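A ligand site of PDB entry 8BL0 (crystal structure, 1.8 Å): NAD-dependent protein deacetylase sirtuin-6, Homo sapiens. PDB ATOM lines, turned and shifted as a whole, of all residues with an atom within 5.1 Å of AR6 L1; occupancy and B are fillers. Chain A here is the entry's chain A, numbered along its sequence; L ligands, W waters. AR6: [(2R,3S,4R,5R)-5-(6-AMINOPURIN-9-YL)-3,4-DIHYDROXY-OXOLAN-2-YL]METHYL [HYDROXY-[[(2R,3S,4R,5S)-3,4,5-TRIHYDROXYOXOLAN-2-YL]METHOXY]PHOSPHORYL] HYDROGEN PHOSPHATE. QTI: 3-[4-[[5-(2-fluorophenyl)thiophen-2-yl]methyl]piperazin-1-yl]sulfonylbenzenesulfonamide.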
ATOM      1  N   GLU A  16       7.611 -13.757  20.281  1.00  0.00           N
ATOM      2  CA  GLU A  16       8.809 -12.921  20.005  1.00  0.00           C
ATOM      3  C   GLU A  16      10.035 -13.822  20.048  1.00  0.00           C
ATOM      4  O   GLU A  16      10.045 -14.804  20.837  1.00  0.00           O
ATOM      5  CB  GLU A  16       8.898 -11.803  21.035  1.00  0.00           C
ATOM      6  CG  GLU A  16       7.839 -10.746  20.842  1.00  0.00           C
ATOM      7  CD  GLU A  16       7.933  -9.612  21.838  1.00  0.00           C
ATOM      8  OE1 GLU A  16       8.498  -9.830  22.915  1.00  0.00           O
ATOM      9  OE2 GLU A  16       7.484  -8.508  21.512  1.00  0.00           O
ATOM     10  N   GLY A  46       7.392   0.057  10.020  1.00  0.00           N
ATOM     11  CA  GLY A  46       6.035  -0.232  10.503  1.00  0.00           C
ATOM     12  C   GLY A  46       5.936   0.141  11.962  1.00  0.00           C
ATOM     13  O   GLY A  46       6.888   0.810  12.473  1.00  0.00           O
ATOM     14  N   ALA A  47       4.857  -0.303  12.596  1.00  0.00           N
ATOM     15  CA  ALA A  47       4.380   0.159  13.920  1.00  0.00           C
ATOM     16  C   ALA A  47       5.417  -0.154  14.997  1.00  0.00           C
ATOM     17  O   ALA A  47       5.466   0.603  16.008  1.00  0.00           O
ATOM     18  CB  ALA A  47       3.020  -0.462  14.199  1.00  0.00           C
ATOM     19  N   GLY A  48       6.281  -1.133  14.768  1.00  0.00           N
ATOM     20  CA  GLY A  48       7.306  -1.566  15.733  1.00  0.00           C
ATOM     21  C   GLY A  48       8.320  -0.468  16.038  1.00  0.00           C
ATOM     22  O   GLY A  48       8.910  -0.504  17.149  1.00  0.00           O
ATOM     23  N   THR A  51       6.808   1.797  19.110  1.00  0.00           N
ATOM     24  CA  THR A  51       6.378   1.153  20.389  1.00  0.00           C
ATOM     25  C   THR A  51       7.176   1.764  21.566  1.00  0.00           C
ATOM     26  O   THR A  51       6.575   1.919  22.681  1.00  0.00           O
ATOM     27  CB  THR A  51       6.434  -0.377  20.359  1.00  0.00           C
ATOM     28  OG1 THR A  51       7.746  -0.811  19.994  1.00  0.00           O
ATOM     29  CG2 THR A  51       5.347  -0.992  19.475  1.00  0.00           C
ATOM     30  N   ASP A  57       1.858  -1.360  18.745  1.00  0.00           N
ATOM     31  CA  ASP A  57       1.833  -1.873  17.344  1.00  0.00           C
ATOM     32  C   ASP A  57       0.460  -2.534  17.073  1.00  0.00           C
ATOM     33  O   ASP A  57      -0.483  -2.332  17.873  1.00  0.00           O
ATOM     34  CB  ASP A  57       3.054  -2.743  17.057  1.00  0.00           C
ATOM     35  CG  ASP A  57       3.144  -4.015  17.898  1.00  0.00           C
ATOM     36  OD1 ASP A  57       2.097  -4.419  18.461  1.00  0.00           O
ATOM     37  OD2 ASP A  57       4.247  -4.580  17.989  1.00  0.00           O
ATOM     38  N   PHE A  58       0.293  -3.196  15.930  1.00  0.00           N
ATOM     39  CA  PHE A  58      -0.981  -3.870  15.555  1.00  0.00           C
ATOM     40  C   PHE A  58      -0.996  -5.349  15.969  1.00  0.00           C
ATOM     41  O   PHE A  58      -2.041  -5.813  16.443  1.00  0.00           O
ATOM     42  CB  PHE A  58      -1.256  -3.668  14.063  1.00  0.00           C
ATOM     43  CG  PHE A  58      -1.620  -2.249  13.760  1.00  0.00           C
ATOM     44  CD1 PHE A  58      -2.929  -1.806  13.898  1.00  0.00           C
ATOM     45  CD2 PHE A  58      -0.639  -1.332  13.385  1.00  0.00           C
ATOM     46  CE1 PHE A  58      -3.261  -0.490  13.624  1.00  0.00           C
ATOM     47  CE2 PHE A  58      -0.973  -0.013  13.143  1.00  0.00           C
ATOM     48  CZ  PHE A  58      -2.281   0.398  13.262  1.00  0.00           C
ATOM     49  N   ARG A  59       0.102  -6.082  15.784  1.00  0.00           N
ATOM     50  CA  ARG A  59       0.092  -7.569  15.798  1.00  0.00           C
ATOM     51  C   ARG A  59       1.133  -8.115  16.775  1.00  0.00           C
ATOM     52  O   ARG A  59       1.229  -9.323  16.891  1.00  0.00           O
ATOM     53  CB  ARG A  59       0.263  -8.159  14.398  1.00  0.00           C
ATOM     54  CG  ARG A  59      -0.841  -7.715  13.441  1.00  0.00           C
ATOM     55  CD  ARG A  59      -0.604  -8.193  12.029  1.00  0.00           C
ATOM     56  NE  ARG A  59      -1.604  -7.612  11.163  1.00  0.00           N
ATOM     57  CZ  ARG A  59      -1.589  -6.376  10.640  1.00  0.00           C
ATOM     58  NH1 ARG A  59      -0.571  -5.553  10.828  1.00  0.00           N
ATOM     59  NH2 ARG A  59      -2.612  -5.992   9.905  1.00  0.00           N
ATOM     60  N   GLY A  60       1.824  -7.247  17.519  1.00  0.00           N
ATOM     61  CA  GLY A  60       2.702  -7.678  18.619  1.00  0.00           C
ATOM     62  C   GLY A  60       1.899  -8.282  19.776  1.00  0.00           C
ATOM     63  O   GLY A  60       0.671  -8.277  19.790  1.00  0.00           O
ATOM     64  N   TRP A  65      -4.751  -5.104  17.184  1.00  0.00           N
ATOM     65  CA  TRP A  65      -5.530  -6.282  16.686  1.00  0.00           C
ATOM     66  C   TRP A  65      -5.385  -7.490  17.633  1.00  0.00           C
ATOM     67  O   TRP A  65      -6.379  -8.197  17.853  1.00  0.00           O
ATOM     68  CB  TRP A  65      -5.114  -6.674  15.269  1.00  0.00           C
ATOM     69  CG  TRP A  65      -5.189  -5.583  14.251  1.00  0.00           C
ATOM     70  CD1 TRP A  65      -4.408  -5.528  13.144  1.00  0.00           C
ATOM     71  CD2 TRP A  65      -6.057  -4.437  14.203  1.00  0.00           C
ATOM     72  NE1 TRP A  65      -4.727  -4.451  12.389  1.00  0.00           N
ATOM     73  CE2 TRP A  65      -5.732  -3.740  13.017  1.00  0.00           C
ATOM     74  CE3 TRP A  65      -7.058  -3.911  15.027  1.00  0.00           C
ATOM     75  CZ2 TRP A  65      -6.368  -2.565  12.636  1.00  0.00           C
ATOM     76  CZ3 TRP A  65      -7.706  -2.754  14.650  1.00  0.00           C
ATOM     77  CH2 TRP A  65      -7.351  -2.081  13.479  1.00  0.00           C
ATOM     78  N   GLN A 107       4.500   2.480   6.728  1.00  0.00           N
ATOM     79  CA  GLN A 107       3.080   2.109   6.891  1.00  0.00           C
ATOM     80  C   GLN A 107       2.496   2.876   8.076  1.00  0.00           C
ATOM     81  O   GLN A 107       1.293   2.736   8.309  1.00  0.00           O
ATOM     82  CB  GLN A 107       2.989   0.585   7.038  1.00  0.00           C
ATOM     83  CG  GLN A 107       3.474  -0.163   5.812  1.00  0.00           C
ATOM     84  CD  GLN A 107       3.621  -1.635   6.107  1.00  0.00           C
ATOM     85  OE1 GLN A 107       2.622  -2.333   6.298  1.00  0.00           O
ATOM     86  NE2 GLN A 107       4.857  -2.105   6.224  1.00  0.00           N
ATOM     87  N   ASN A 108       3.296   3.686   8.788  1.00  0.00           N
ATOM     88  CA  ASN A 108       2.869   4.377  10.035  1.00  0.00           C
ATOM     89  C   ASN A 108       2.070   5.649   9.696  1.00  0.00           C
ATOM     90  O   ASN A 108       2.452   6.413   8.769  1.00  0.00           O
ATOM     91  CB  ASN A 108       4.050   4.679  10.958  1.00  0.00           C
ATOM     92  CG  ASN A 108       4.710   3.407  11.421  1.00  0.00           C
ATOM     93  OD1 ASN A 108       4.167   2.308  11.234  1.00  0.00           O
ATOM     94  ND2 ASN A 108       5.900   3.543  11.983  1.00  0.00           N
ATOM     95  N   HIS A 127       0.013   4.595   4.128  1.00  0.00           N
ATOM     96  CA  HIS A 127      -1.294   4.391   4.831  1.00  0.00           C
ATOM     97  C   HIS A 127      -1.829   5.729   5.363  1.00  0.00           C
ATOM     98  O   HIS A 127      -2.925   5.741   5.973  1.00  0.00           O
ATOM     99  CB  HIS A 127      -1.188   3.305   5.943  1.00  0.00           C
ATOM    100  CG  HIS A 127      -0.746   1.954   5.464  1.00  0.00           C
ATOM    101  ND1 HIS A 127      -0.418   0.898   6.339  1.00  0.00           N
ATOM    102  CD2 HIS A 127      -0.600   1.472   4.207  1.00  0.00           C
ATOM    103  CE1 HIS A 127      -0.065  -0.149   5.625  1.00  0.00           C
ATOM    104  NE2 HIS A 127      -0.189   0.180   4.307  1.00  0.00           N
ATOM    105  N   TRP A 182      -9.682   0.044   5.308  1.00  0.00           N
ATOM    106  CA  TRP A 182      -9.370  -1.321   4.818  1.00  0.00           C
ATOM    107  C   TRP A 182      -9.524  -1.433   3.298  1.00  0.00           C
ATOM    108  O   TRP A 182      -8.639  -2.065   2.683  1.00  0.00           O
ATOM    109  CB  TRP A 182     -10.250  -2.350   5.547  1.00  0.00           C
ATOM    110  CG  TRP A 182      -9.789  -2.565   6.955  1.00  0.00           C
ATOM    111  CD1 TRP A 182     -10.315  -2.023   8.090  1.00  0.00           C
ATOM    112  CD2 TRP A 182      -8.662  -3.357   7.363  1.00  0.00           C
ATOM    113  NE1 TRP A 182      -9.600  -2.432   9.185  1.00  0.00           N
ATOM    114  CE2 TRP A 182      -8.584  -3.246   8.777  1.00  0.00           C
ATOM    115  CE3 TRP A 182      -7.733  -4.154   6.687  1.00  0.00           C
ATOM    116  CZ2 TRP A 182      -7.606  -3.917   9.510  1.00  0.00           C
ATOM    117  CZ3 TRP A 182      -6.762  -4.804   7.420  1.00  0.00           C
ATOM    118  CH2 TRP A 182      -6.696  -4.682   8.815  1.00  0.00           C
ATOM    119  N   GLY A 208      10.592  -3.105  12.353  1.00  0.00           N
ATOM    120  CA  GLY A 208       9.324  -3.208  13.112  1.00  0.00           C
ATOM    121  C   GLY A 208       8.107  -3.249  12.222  1.00  0.00           C
ATOM    122  O   GLY A 208       7.165  -2.498  12.493  1.00  0.00           O
ATOM    123  N   THR A 209       8.121  -4.078  11.171  1.00  0.00           N
ATOM    124  CA  THR A 209       6.929  -4.428  10.376  1.00  0.00           C
ATOM    125  C   THR A 209       6.877  -5.949  10.175  1.00  0.00           C
ATOM    126  O   THR A 209       7.933  -6.569   9.951  1.00  0.00           O
ATOM    127  CB  THR A 209       6.888  -3.675   9.043  1.00  0.00           C
ATOM    128  OG1 THR A 209       5.746  -4.184   8.350  1.00  0.00           O
ATOM    129  CG2 THR A 209       8.144  -3.873   8.203  1.00  0.00           C
ATOM    130  N   SER A 210       5.669  -6.547  10.284  1.00  0.00           N
ATOM    131  CA  SER A 210       5.465  -8.011  10.155  1.00  0.00           C
ATOM    132  C   SER A 210       5.231  -8.351   8.667  1.00  0.00           C
ATOM    133  O   SER A 210       5.192  -9.551   8.351  1.00  0.00           O
ATOM    134  CB  SER A 210       4.349  -8.536  11.060  1.00  0.00           C
ATOM    135  OG  SER A 210       3.072  -7.997  10.753  1.00  0.00           O
ATOM    136  N   LEU A 211       5.102  -7.319   7.820  1.00  0.00           N
ATOM    137  CA  LEU A 211       5.122  -7.401   6.320  1.00  0.00           C
ATOM    138  C   LEU A 211       3.902  -8.168   5.784  1.00  0.00           C
ATOM    139  O   LEU A 211       3.981  -8.787   4.695  1.00  0.00           O
ATOM    140  CB  LEU A 211       6.447  -8.028   5.861  1.00  0.00           C
ATOM    141  CG  LEU A 211       7.715  -7.252   6.231  1.00  0.00           C
ATOM    142  CD1 LEU A 211       8.959  -8.077   5.926  1.00  0.00           C
ATOM    143  CD2 LEU A 211       7.775  -5.909   5.506  1.00  0.00           C
ATOM    144  N   GLN A 212       2.777  -8.091   6.500  1.00  0.00           N
ATOM    145  CA  GLN A 212       1.571  -8.909   6.210  1.00  0.00           C
ATOM    146  C   GLN A 212       0.615  -8.157   5.282  1.00  0.00           C
ATOM    147  O   GLN A 212      -0.347  -8.798   4.844  1.00  0.00           O
ATOM    148  CB  GLN A 212       0.862  -9.290   7.496  1.00  0.00           C
ATOM    149  CG  GLN A 212       1.687 -10.189   8.402  1.00  0.00           C
ATOM    150  CD  GLN A 212       0.872 -10.764   9.529  1.00  0.00           C
ATOM    151  OE1 GLN A 212      -0.147 -11.417   9.310  1.00  0.00           O
ATOM    152  NE2 GLN A 212       1.340 -10.550  10.755  1.00  0.00           N
ATOM    153  N   ILE A 213       0.802  -6.845   5.065  1.00  0.00           N
ATOM    154  CA  ILE A 213      -0.162  -5.994   4.318  1.00  0.00           C
ATOM    155  C   ILE A 213       0.368  -5.783   2.898  1.00  0.00           C
ATOM    156  O   ILE A 213       1.492  -5.288   2.764  1.00  0.00           O
ATOM    157  CB  ILE A 213      -0.430  -4.636   5.013  1.00  0.00           C
ATOM    158  CG1 ILE A 213      -1.054  -4.818   6.401  1.00  0.00           C
ATOM    159  CG2 ILE A 213      -1.304  -3.750   4.130  1.00  0.00           C
ATOM    160  CD1 ILE A 213      -2.493  -5.244   6.377  1.00  0.00           C
ATOM    161  N   VAL A 233      14.578  -6.546  10.350  1.00  0.00           N
ATOM    162  CA  VAL A 233      14.747  -6.330  11.819  1.00  0.00           C
ATOM    163  C   VAL A 233      13.351  -6.355  12.459  1.00  0.00           C
ATOM    164  O   VAL A 233      12.513  -5.492  12.134  1.00  0.00           O
ATOM    165  CB  VAL A 233      15.495  -5.023  12.131  1.00  0.00           C
ATOM    166  CG1 VAL A 233      15.716  -4.852  13.632  1.00  0.00           C
ATOM    167  CG2 VAL A 233      16.808  -4.896  11.370  1.00  0.00           C
ATOM    168  N   ASN A 234      13.107  -7.314  13.346  1.00  0.00           N
ATOM    169  CA  ASN A 234      11.747  -7.543  13.918  1.00  0.00           C
ATOM    170  C   ASN A 234      11.808  -8.559  15.057  1.00  0.00           C
ATOM    171  O   ASN A 234      12.504  -9.590  14.901  1.00  0.00           O
ATOM    172  CB  ASN A 234      10.772  -8.058  12.858  1.00  0.00           C
ATOM    173  CG  ASN A 234       9.363  -7.579  13.130  1.00  0.00           C
ATOM    174  OD1 ASN A 234       9.097  -6.367  13.136  1.00  0.00           O
ATOM    175  ND2 ASN A 234       8.449  -8.513  13.306  1.00  0.00           N
ATOM    176  N   LEU A 235      11.087  -8.279  16.151  1.00  0.00           N
ATOM    177  CA  LEU A 235      10.984  -9.180  17.310  1.00  0.00           C
ATOM    178  C   LEU A 235      10.207 -10.477  16.952  1.00  0.00           C
ATOM    179  O   LEU A 235      10.622 -11.565  17.398  1.00  0.00           O
ATOM    180  CB  LEU A 235      10.320  -8.415  18.462  1.00  0.00           C
ATOM    181  CG  LEU A 235      11.210  -7.415  19.172  1.00  0.00           C
ATOM    182  CD1 LEU A 235      10.409  -6.661  20.223  1.00  0.00           C
ATOM    183  CD2 LEU A 235      12.423  -8.097  19.801  1.00  0.00           C
ATOM    184  N   GLN A 236       9.132 -10.364  16.174  1.00  0.00           N
ATOM    185  CA  GLN A 236       8.290 -11.507  15.739  1.00  0.00           C
ATOM    186  C   GLN A 236       8.742 -11.962  14.349  1.00  0.00           C
ATOM    187  O   GLN A 236       9.402 -11.217  13.617  1.00  0.00           O
ATOM    188  CB  GLN A 236       6.824 -11.108  15.619  1.00  0.00           C
ATOM    189  CG  GLN A 236       6.107 -10.928  16.943  1.00  0.00           C
ATOM    190  CD  GLN A 236       4.692 -10.450  16.764  1.00  0.00           C
ATOM    191  OE1 GLN A 236       4.369  -9.660  15.864  1.00  0.00           O
ATOM    192  NE2 GLN A 236       3.794 -10.917  17.626  1.00  0.00           N
ATOM    193  N   PRO A 237       8.342 -13.181  13.952  1.00  0.00           N
ATOM    194  CA  PRO A 237       8.406 -13.594  12.555  1.00  0.00           C
ATOM    195  C   PRO A 237       7.642 -12.601  11.670  1.00  0.00           C
ATOM    196  O   PRO A 237       6.715 -11.947  12.129  1.00  0.00           O
ATOM    197  CB  PRO A 237       7.675 -14.960  12.499  1.00  0.00           C
ATOM    198  CG  PRO A 237       7.645 -15.440  13.934  1.00  0.00           C
ATOM    199  CD  PRO A 237       7.790 -14.231  14.822  1.00  0.00           C
ATOM    200  N   GLY A 250      15.651  -8.404  17.600  1.00  0.00           N
ATOM    201  CA  GLY A 250      16.065  -7.514  18.714  1.00  0.00           C
ATOM    202  C   GLY A 250      15.254  -6.232  18.686  1.00  0.00           C
ATOM    203  O   GLY A 250      14.508  -6.032  17.693  1.00  0.00           O
ATOM    204  N   TYR A 251      15.322  -5.442  19.762  1.00  0.00           N
ATOM    205  CA  TYR A 251      14.669  -4.113  19.807  1.00  0.00           C
ATOM    206  C   TYR A 251      15.317  -3.236  18.741  1.00  0.00           C
ATOM    207  O   TYR A 251      16.581  -3.191  18.664  1.00  0.00           O
ATOM    208  CB  TYR A 251      14.709  -3.501  21.209  1.00  0.00           C
ATOM    209  CG  TYR A 251      13.936  -4.338  22.199  1.00  0.00           C
ATOM    210  CD1 TYR A 251      12.569  -4.169  22.358  1.00  0.00           C
ATOM    211  CD2 TYR A 251      14.559  -5.324  22.951  1.00  0.00           C
ATOM    212  CE1 TYR A 251      11.841  -4.929  23.261  1.00  0.00           C
ATOM    213  CE2 TYR A 251      13.847  -6.097  23.841  1.00  0.00           C
ATOM    214  CZ  TYR A 251      12.489  -5.911  23.986  1.00  0.00           C
ATOM    215  OH  TYR A 251      11.790  -6.666  24.872  1.00  0.00           O
ATOM    216  N   VAL A 252      14.497  -2.573  17.931  1.00  0.00           N
ATOM    217  CA  VAL A 252      15.002  -1.775  16.789  1.00  0.00           C
ATOM    218  C   VAL A 252      15.874  -0.628  17.309  1.00  0.00           C
ATOM    219  O   VAL A 252      16.906  -0.369  16.686  1.00  0.00           O
ATOM    220  CB  VAL A 252      13.890  -1.319  15.833  1.00  0.00           C
ATOM    221  CG1 VAL A 252      12.867  -0.379  16.502  1.00  0.00           C
ATOM    222  CG2 VAL A 252      14.506  -0.695  14.615  1.00  0.00           C
HETATM  223  N1  AR6 L   1      11.760  -3.551  18.044  1.00  0.00           N
HETATM  224  C2  AR6 L   1      11.582  -4.488  17.095  1.00  0.00           C
HETATM  225  N3  AR6 L   1      10.438  -5.014  16.639  1.00  0.00           N
HETATM  226  C4  AR6 L   1       9.373  -4.478  17.261  1.00  0.00           C
HETATM  227  C5  AR6 L   1       9.399  -3.546  18.276  1.00  0.00           C
HETATM  228  C6  AR6 L   1      10.660  -3.060  18.676  1.00  0.00           C
HETATM  229  N6  AR6 L   1      10.814  -2.131  19.620  1.00  0.00           N
HETATM  230  N7  AR6 L   1       8.106  -3.252  18.687  1.00  0.00           N
HETATM  231  C8  AR6 L   1       7.330  -3.988  17.934  1.00  0.00           C
HETATM  232  N9  AR6 L   1       8.051  -4.775  17.058  1.00  0.00           N
HETATM  233  PA  AR6 L   1       2.515  -5.034  12.915  1.00  0.00           P
HETATM  234  PB  AR6 L   1       2.780  -3.171  10.682  1.00  0.00           P
HETATM  235  C1' AR6 L   1       7.551  -5.637  16.003  1.00  0.00           C
HETATM  236  O1A AR6 L   1       1.926  -6.026  11.971  1.00  0.00           O
HETATM  237  O1B AR6 L   1       3.308  -1.772  10.587  1.00  0.00           O
HETATM  238  C1D AR6 L   1      -2.326  -2.413  10.232  1.00  0.00           C
HETATM  239  O1D AR6 L   1      -3.655  -2.824   9.986  1.00  0.00           O
HETATM  240  C2' AR6 L   1       6.458  -6.646  16.317  1.00  0.00           C
HETATM  241  O2' AR6 L   1       7.052  -7.868  16.679  1.00  0.00           O
HETATM  242  O2A AR6 L   1       2.004  -4.815  14.303  1.00  0.00           O
HETATM  243  O2B AR6 L   1       3.535  -4.246  10.022  1.00  0.00           O
HETATM  244  C2D AR6 L   1      -2.090  -0.928   9.879  1.00  0.00           C
HETATM  245  O2D AR6 L   1      -2.821  -0.499   8.745  1.00  0.00           O
HETATM  246  C3' AR6 L   1       5.669  -6.744  15.003  1.00  0.00           C
HETATM  247  O3' AR6 L   1       5.903  -7.938  14.274  1.00  0.00           O
HETATM  248  O3A AR6 L   1       2.531  -3.570  12.234  1.00  0.00           O
HETATM  249  C3D AR6 L   1      -0.588  -0.900   9.626  1.00  0.00           C
HETATM  250  O3D AR6 L   1      -0.079   0.228   8.883  1.00  0.00           O
HETATM  251  C4' AR6 L   1       6.096  -5.509  14.191  1.00  0.00           C
HETATM  252  O4' AR6 L   1       7.017  -4.774  15.034  1.00  0.00           O
HETATM  253  C4D AR6 L   1      -0.445  -2.209   8.842  1.00  0.00           C
HETATM  254  O4D AR6 L   1      -1.419  -3.130   9.401  1.00  0.00           O
HETATM  255  C5' AR6 L   1       4.966  -4.591  13.816  1.00  0.00           C
HETATM  256  O5' AR6 L   1       4.069  -5.347  13.000  1.00  0.00           O
HETATM  257  C5D AR6 L   1       0.910  -2.874   8.882  1.00  0.00           C
HETATM  258  O5D AR6 L   1       1.242  -3.164  10.273  1.00  0.00           O
HETATM  259  C10 QTI L   2      -1.385   3.971  14.724  1.00  0.00           C
HETATM  260  C15 QTI L   2      -5.742   2.366  14.692  1.00  0.00           C
HETATM  261  C20 QTI L   2      -8.102   1.421   8.991  1.00  0.00           C
HETATM  262  C21 QTI L   2      -7.556   0.991   7.773  1.00  0.00           C
HETATM  263  C22 QTI L   2      -6.345   0.296   7.837  1.00  0.00           C
HETATM  264  C24 QTI L   2      -5.624  -0.220   6.718  1.00  0.00           C
HETATM  265  C26 QTI L   2      -4.741   0.138   4.448  1.00  0.00           C
HETATM  266  C28 QTI L   2      -4.339  -1.971   5.557  1.00  0.00           C
HETATM  267  N01 QTI L   2       1.496   2.329  12.924  1.00  0.00           N
HETATM  268  S02 QTI L   2       1.261   3.618  14.007  1.00  0.00           S
HETATM  269  O03 QTI L   2       1.002   4.932  13.172  1.00  0.00           O
HETATM  270  O04 QTI L   2       2.490   3.798  14.999  1.00  0.00           O
HETATM  271  C05 QTI L   2      -0.192   3.254  14.958  1.00  0.00           C
HETATM  272  C06 QTI L   2      -0.151   2.214  15.929  1.00  0.00           C
HETATM  273  C07 QTI L   2      -1.313   1.916  16.697  1.00  0.00           C
HETATM  274  C08 QTI L   2      -2.505   2.642  16.462  1.00  0.00           C
HETATM  275  C09 QTI L   2      -2.553   3.661  15.474  1.00  0.00           C
HETATM  276  S11 QTI L   2      -4.076   4.519  15.193  1.00  0.00           S
HETATM  277  O12 QTI L   2      -4.764   4.646  16.638  1.00  0.00           O
HETATM  278  O13 QTI L   2      -3.768   5.932  14.602  1.00  0.00           O
HETATM  279  N14 QTI L   2      -5.140   3.598  14.107  1.00  0.00           N
HETATM  280  C16 QTI L   2      -6.932   1.947  13.809  1.00  0.00           C
HETATM  281  N17 QTI L   2      -6.535   1.838  12.347  1.00  0.00           N
HETATM  282  C18 QTI L   2      -7.704   1.421  11.511  1.00  0.00           C
HETATM  283  C19 QTI L   2      -7.354   1.102  10.125  1.00  0.00           C
HETATM  284  S23 QTI L   2      -5.947   0.221   9.560  1.00  0.00           S
HETATM  285  C25 QTI L   2      -5.448   0.592   5.578  1.00  0.00           C
HETATM  286  C27 QTI L   2      -4.189  -1.154   4.433  1.00  0.00           C
HETATM  287  C29 QTI L   2      -5.047  -1.527   6.688  1.00  0.00           C
HETATM  288  F30 QTI L   2      -5.148  -2.350   7.708  1.00  0.00           F
HETATM  289  C31 QTI L   2      -5.916   3.104  11.818  1.00  0.00           C
HETATM  290  C32 QTI L   2      -4.713   3.569  12.675  1.00  0.00           C
HETATM  291  O   HOH W   1       5.184  -5.585  20.191  1.00  0.00           O
HETATM  292  O   HOH W   2      13.022  -0.092  19.789  1.00  0.00           O
HETATM  293  O   HOH W   3      -0.272   2.901  10.641  1.00  0.00           O
HETATM  294  O   HOH W   4       6.676  -7.959  19.278  1.00  0.00           O
HETATM  295  O   HOH W   5      10.209   1.066  19.127  1.00  0.00           O
HETATM  296  O   HOH W   6       2.104  -6.304   8.824  1.00  0.00           O
HETATM  297  O   HOH W   7       1.997   0.592  10.677  1.00  0.00           O
HETATM  298  O   HOH W   8      -3.092   2.078   9.036  1.00  0.00           O
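N7 of AR6 L1 sits close to O of Gly 48. An oxygen (O4') of AR6 L1 lies close to the backbone carbonyl oxygen (O) of Gly 208, 3.4 Å away. CA of Gly 46 touches O1B of AR6 L1, at 3.1 Å. Asp 57 touches AR6 L1. Trp 182 touches AR6 L1 (CH2 to O1D, 3.8 Å). CG1 of Ile 213 touches O4D of AR6 L1, 3.5 Å away. O of Gly 250 touches C2 of AR6 L1, 3.4 Å away. CA of Tyr 251 touches N1 of AR6 L1, at 3.4 Å. Hydrophobic or aromatic side chains that line AR6 L1: Ala 47, Phe 58, Trp 65, His 127, Trp 182, Ile 213, Leu 235, Tyr 251 and Val 252. 21 residues have an atom within 4 Å of AR6 L1: Gly 46, Ala 47, Gly 48, Thr 51, Asp 57, Phe 58, Arg 59, Trp 65, Gln 107, His 127, Trp 182, Gly 208, Thr 209, Ser 210, Ile 213, Asn 234, Leu 235, Gln 236, Gly 250, Tyr 251 and Val 252.
An oxygen (O2D) of AR6 L1 lies close to a sulfur (S23) of QTI L2 (3.3 Å).
The backbone NH (N) of Ser 210 is in hydrogen-bond range of an oxygen (O2B) of AR6 L1 (3.1 Å). OG of Ser 210 lies within hydrogen-bond range of O1A of AR6 L1, 2.6 Å away. An oxygen (O3D) of AR6 L1 is in hydrogen-bond range of a ring nitrogen (ND1) of His 127, 2.7 Å away. O2A of AR6 L1 is in hydrogen-bond range of N of Arg 59. An oxygen (O1A) of AR6 L1 is in salt-bridge range of the guanidinium group of Arg 59, at 2.8 Å. An oxygen (O2B) of AR6 L1 sits at hydrogen-bond distance from the side-chain hydroxyl of Thr 209, at 2.8 Å. The side-chain amide nitrogen (ND2) of Asn 234 is in hydrogen-bond range of an oxygen (O3') of AR6 L1 (2.8 Å). A nitrogen (N7) of AR6 L1 sits at hydrogen-bond distance from the side-chain hydroxyl of Thr 51, 2.8 Å away. The backbone NH (N) of Gln 236 lies close to an oxygen (O2') of AR6 L1. The side-chain amide oxygen (OE1) of Gln 236 lies within hydrogen-bond range of an oxygen (O3') of AR6 L1 (2.8 Å). O2A of AR6 L1 lies within hydrogen-bond range of N of Phe 58. The backbone NH (N) of Val 252 lies within hydrogen-bond range of a nitrogen (N1) of AR6 L1 (2.9 Å). An oxygen (O3D) of AR6 L1 lies within hydrogen-bond range of the backbone carbonyl oxygen of Gln 107, 2.9 Å away. An oxygen (O1B) of AR6 L1 sits at hydrogen-bond distance from the backbone NH (N) of Ala 47 (2.9 Å). The indole nitrogen of Trp 65 is in hydrogen-bond range of an oxygen (O1D) of AR6 L1 (3.1 Å). N of Leu 235 lies within hydrogen-bond range of N3 of AR6 L1 (3.4 Å). The side-chain amide oxygen (OD1) of Asn 108 is in hydrogen-bond range of a nitrogen (N01) of QTI L2, at 3.2 Å.
Water W8 lies within hydrogen-bond range of O2D of AR6 L1 and S23 of QTI L2. Water W4 bridges the side-chain carboxylate of Glu 16 and an oxygen (O2') of AR6 L1. Water W7 lies within hydrogen-bond range of an oxygen (O1B) of AR6 L1, the side-chain amide oxygen of Asn 108, a nitrogen (N01) of QTI L2 and the backbone carbonyl oxygen of Gln 107. Water W2 bridges a nitrogen (N6) of AR6 L1 (3.0 Å) and the backbone NH of Val 252 (3.4 Å). Water W3 lies within hydrogen-bond range of O of Gln 107 (2.8 Å), N01 of QTI L2 (2.9 Å) and O3D of AR6 L1 (3.2 Å). Water W5 lies within hydrogen-bond range of the backbone carbonyl oxygen (O) of Gly 48 (2.8 Å), the side-chain hydroxyl (OG1) of Thr 51 (3.2 Å) and a nitrogen (N6) of AR6 L1 (3.3 Å).
The side-chain hydroxyl (OG) of Ser 210 lies within hydrogen-bond range of the side-chain amide nitrogen (NE2) of Gln 212 (3.1 Å). A ring nitrogen (ND1) of His 127 sits at hydrogen-bond distance from the backbone carbonyl oxygen (O) of Gln 107 (3.2 Å). The side-chain amide nitrogen (NE2) of Gln 107 sits at hydrogen-bond distance from the side-chain hydroxyl (OG1) of Thr 209, at 3.1 Å. The backbone carbonyl oxygen (O) of Gln 236 is in hydrogen-bond range of the side-chain amide nitrogen (ND2) of Asn 234 (2.9 Å). The side-chain hydroxyl of Thr 51 sits at hydrogen-bond distance from the backbone carbonyl oxygen of Gly 48 (3.1 Å). The backbone carbonyl oxygen (O) of Gly 46 sits at hydrogen-bond distance from the side-chain amide nitrogen (ND2) of Asn 108 (2.9 Å). OD1 of Asp 57 is in hydrogen-bond range of N of Gly 60, at 3.0 Å. The backbone carbonyl oxygen of Val 233 is in hydrogen-bond range of the backbone NH of Gly 208 (3.1 Å).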
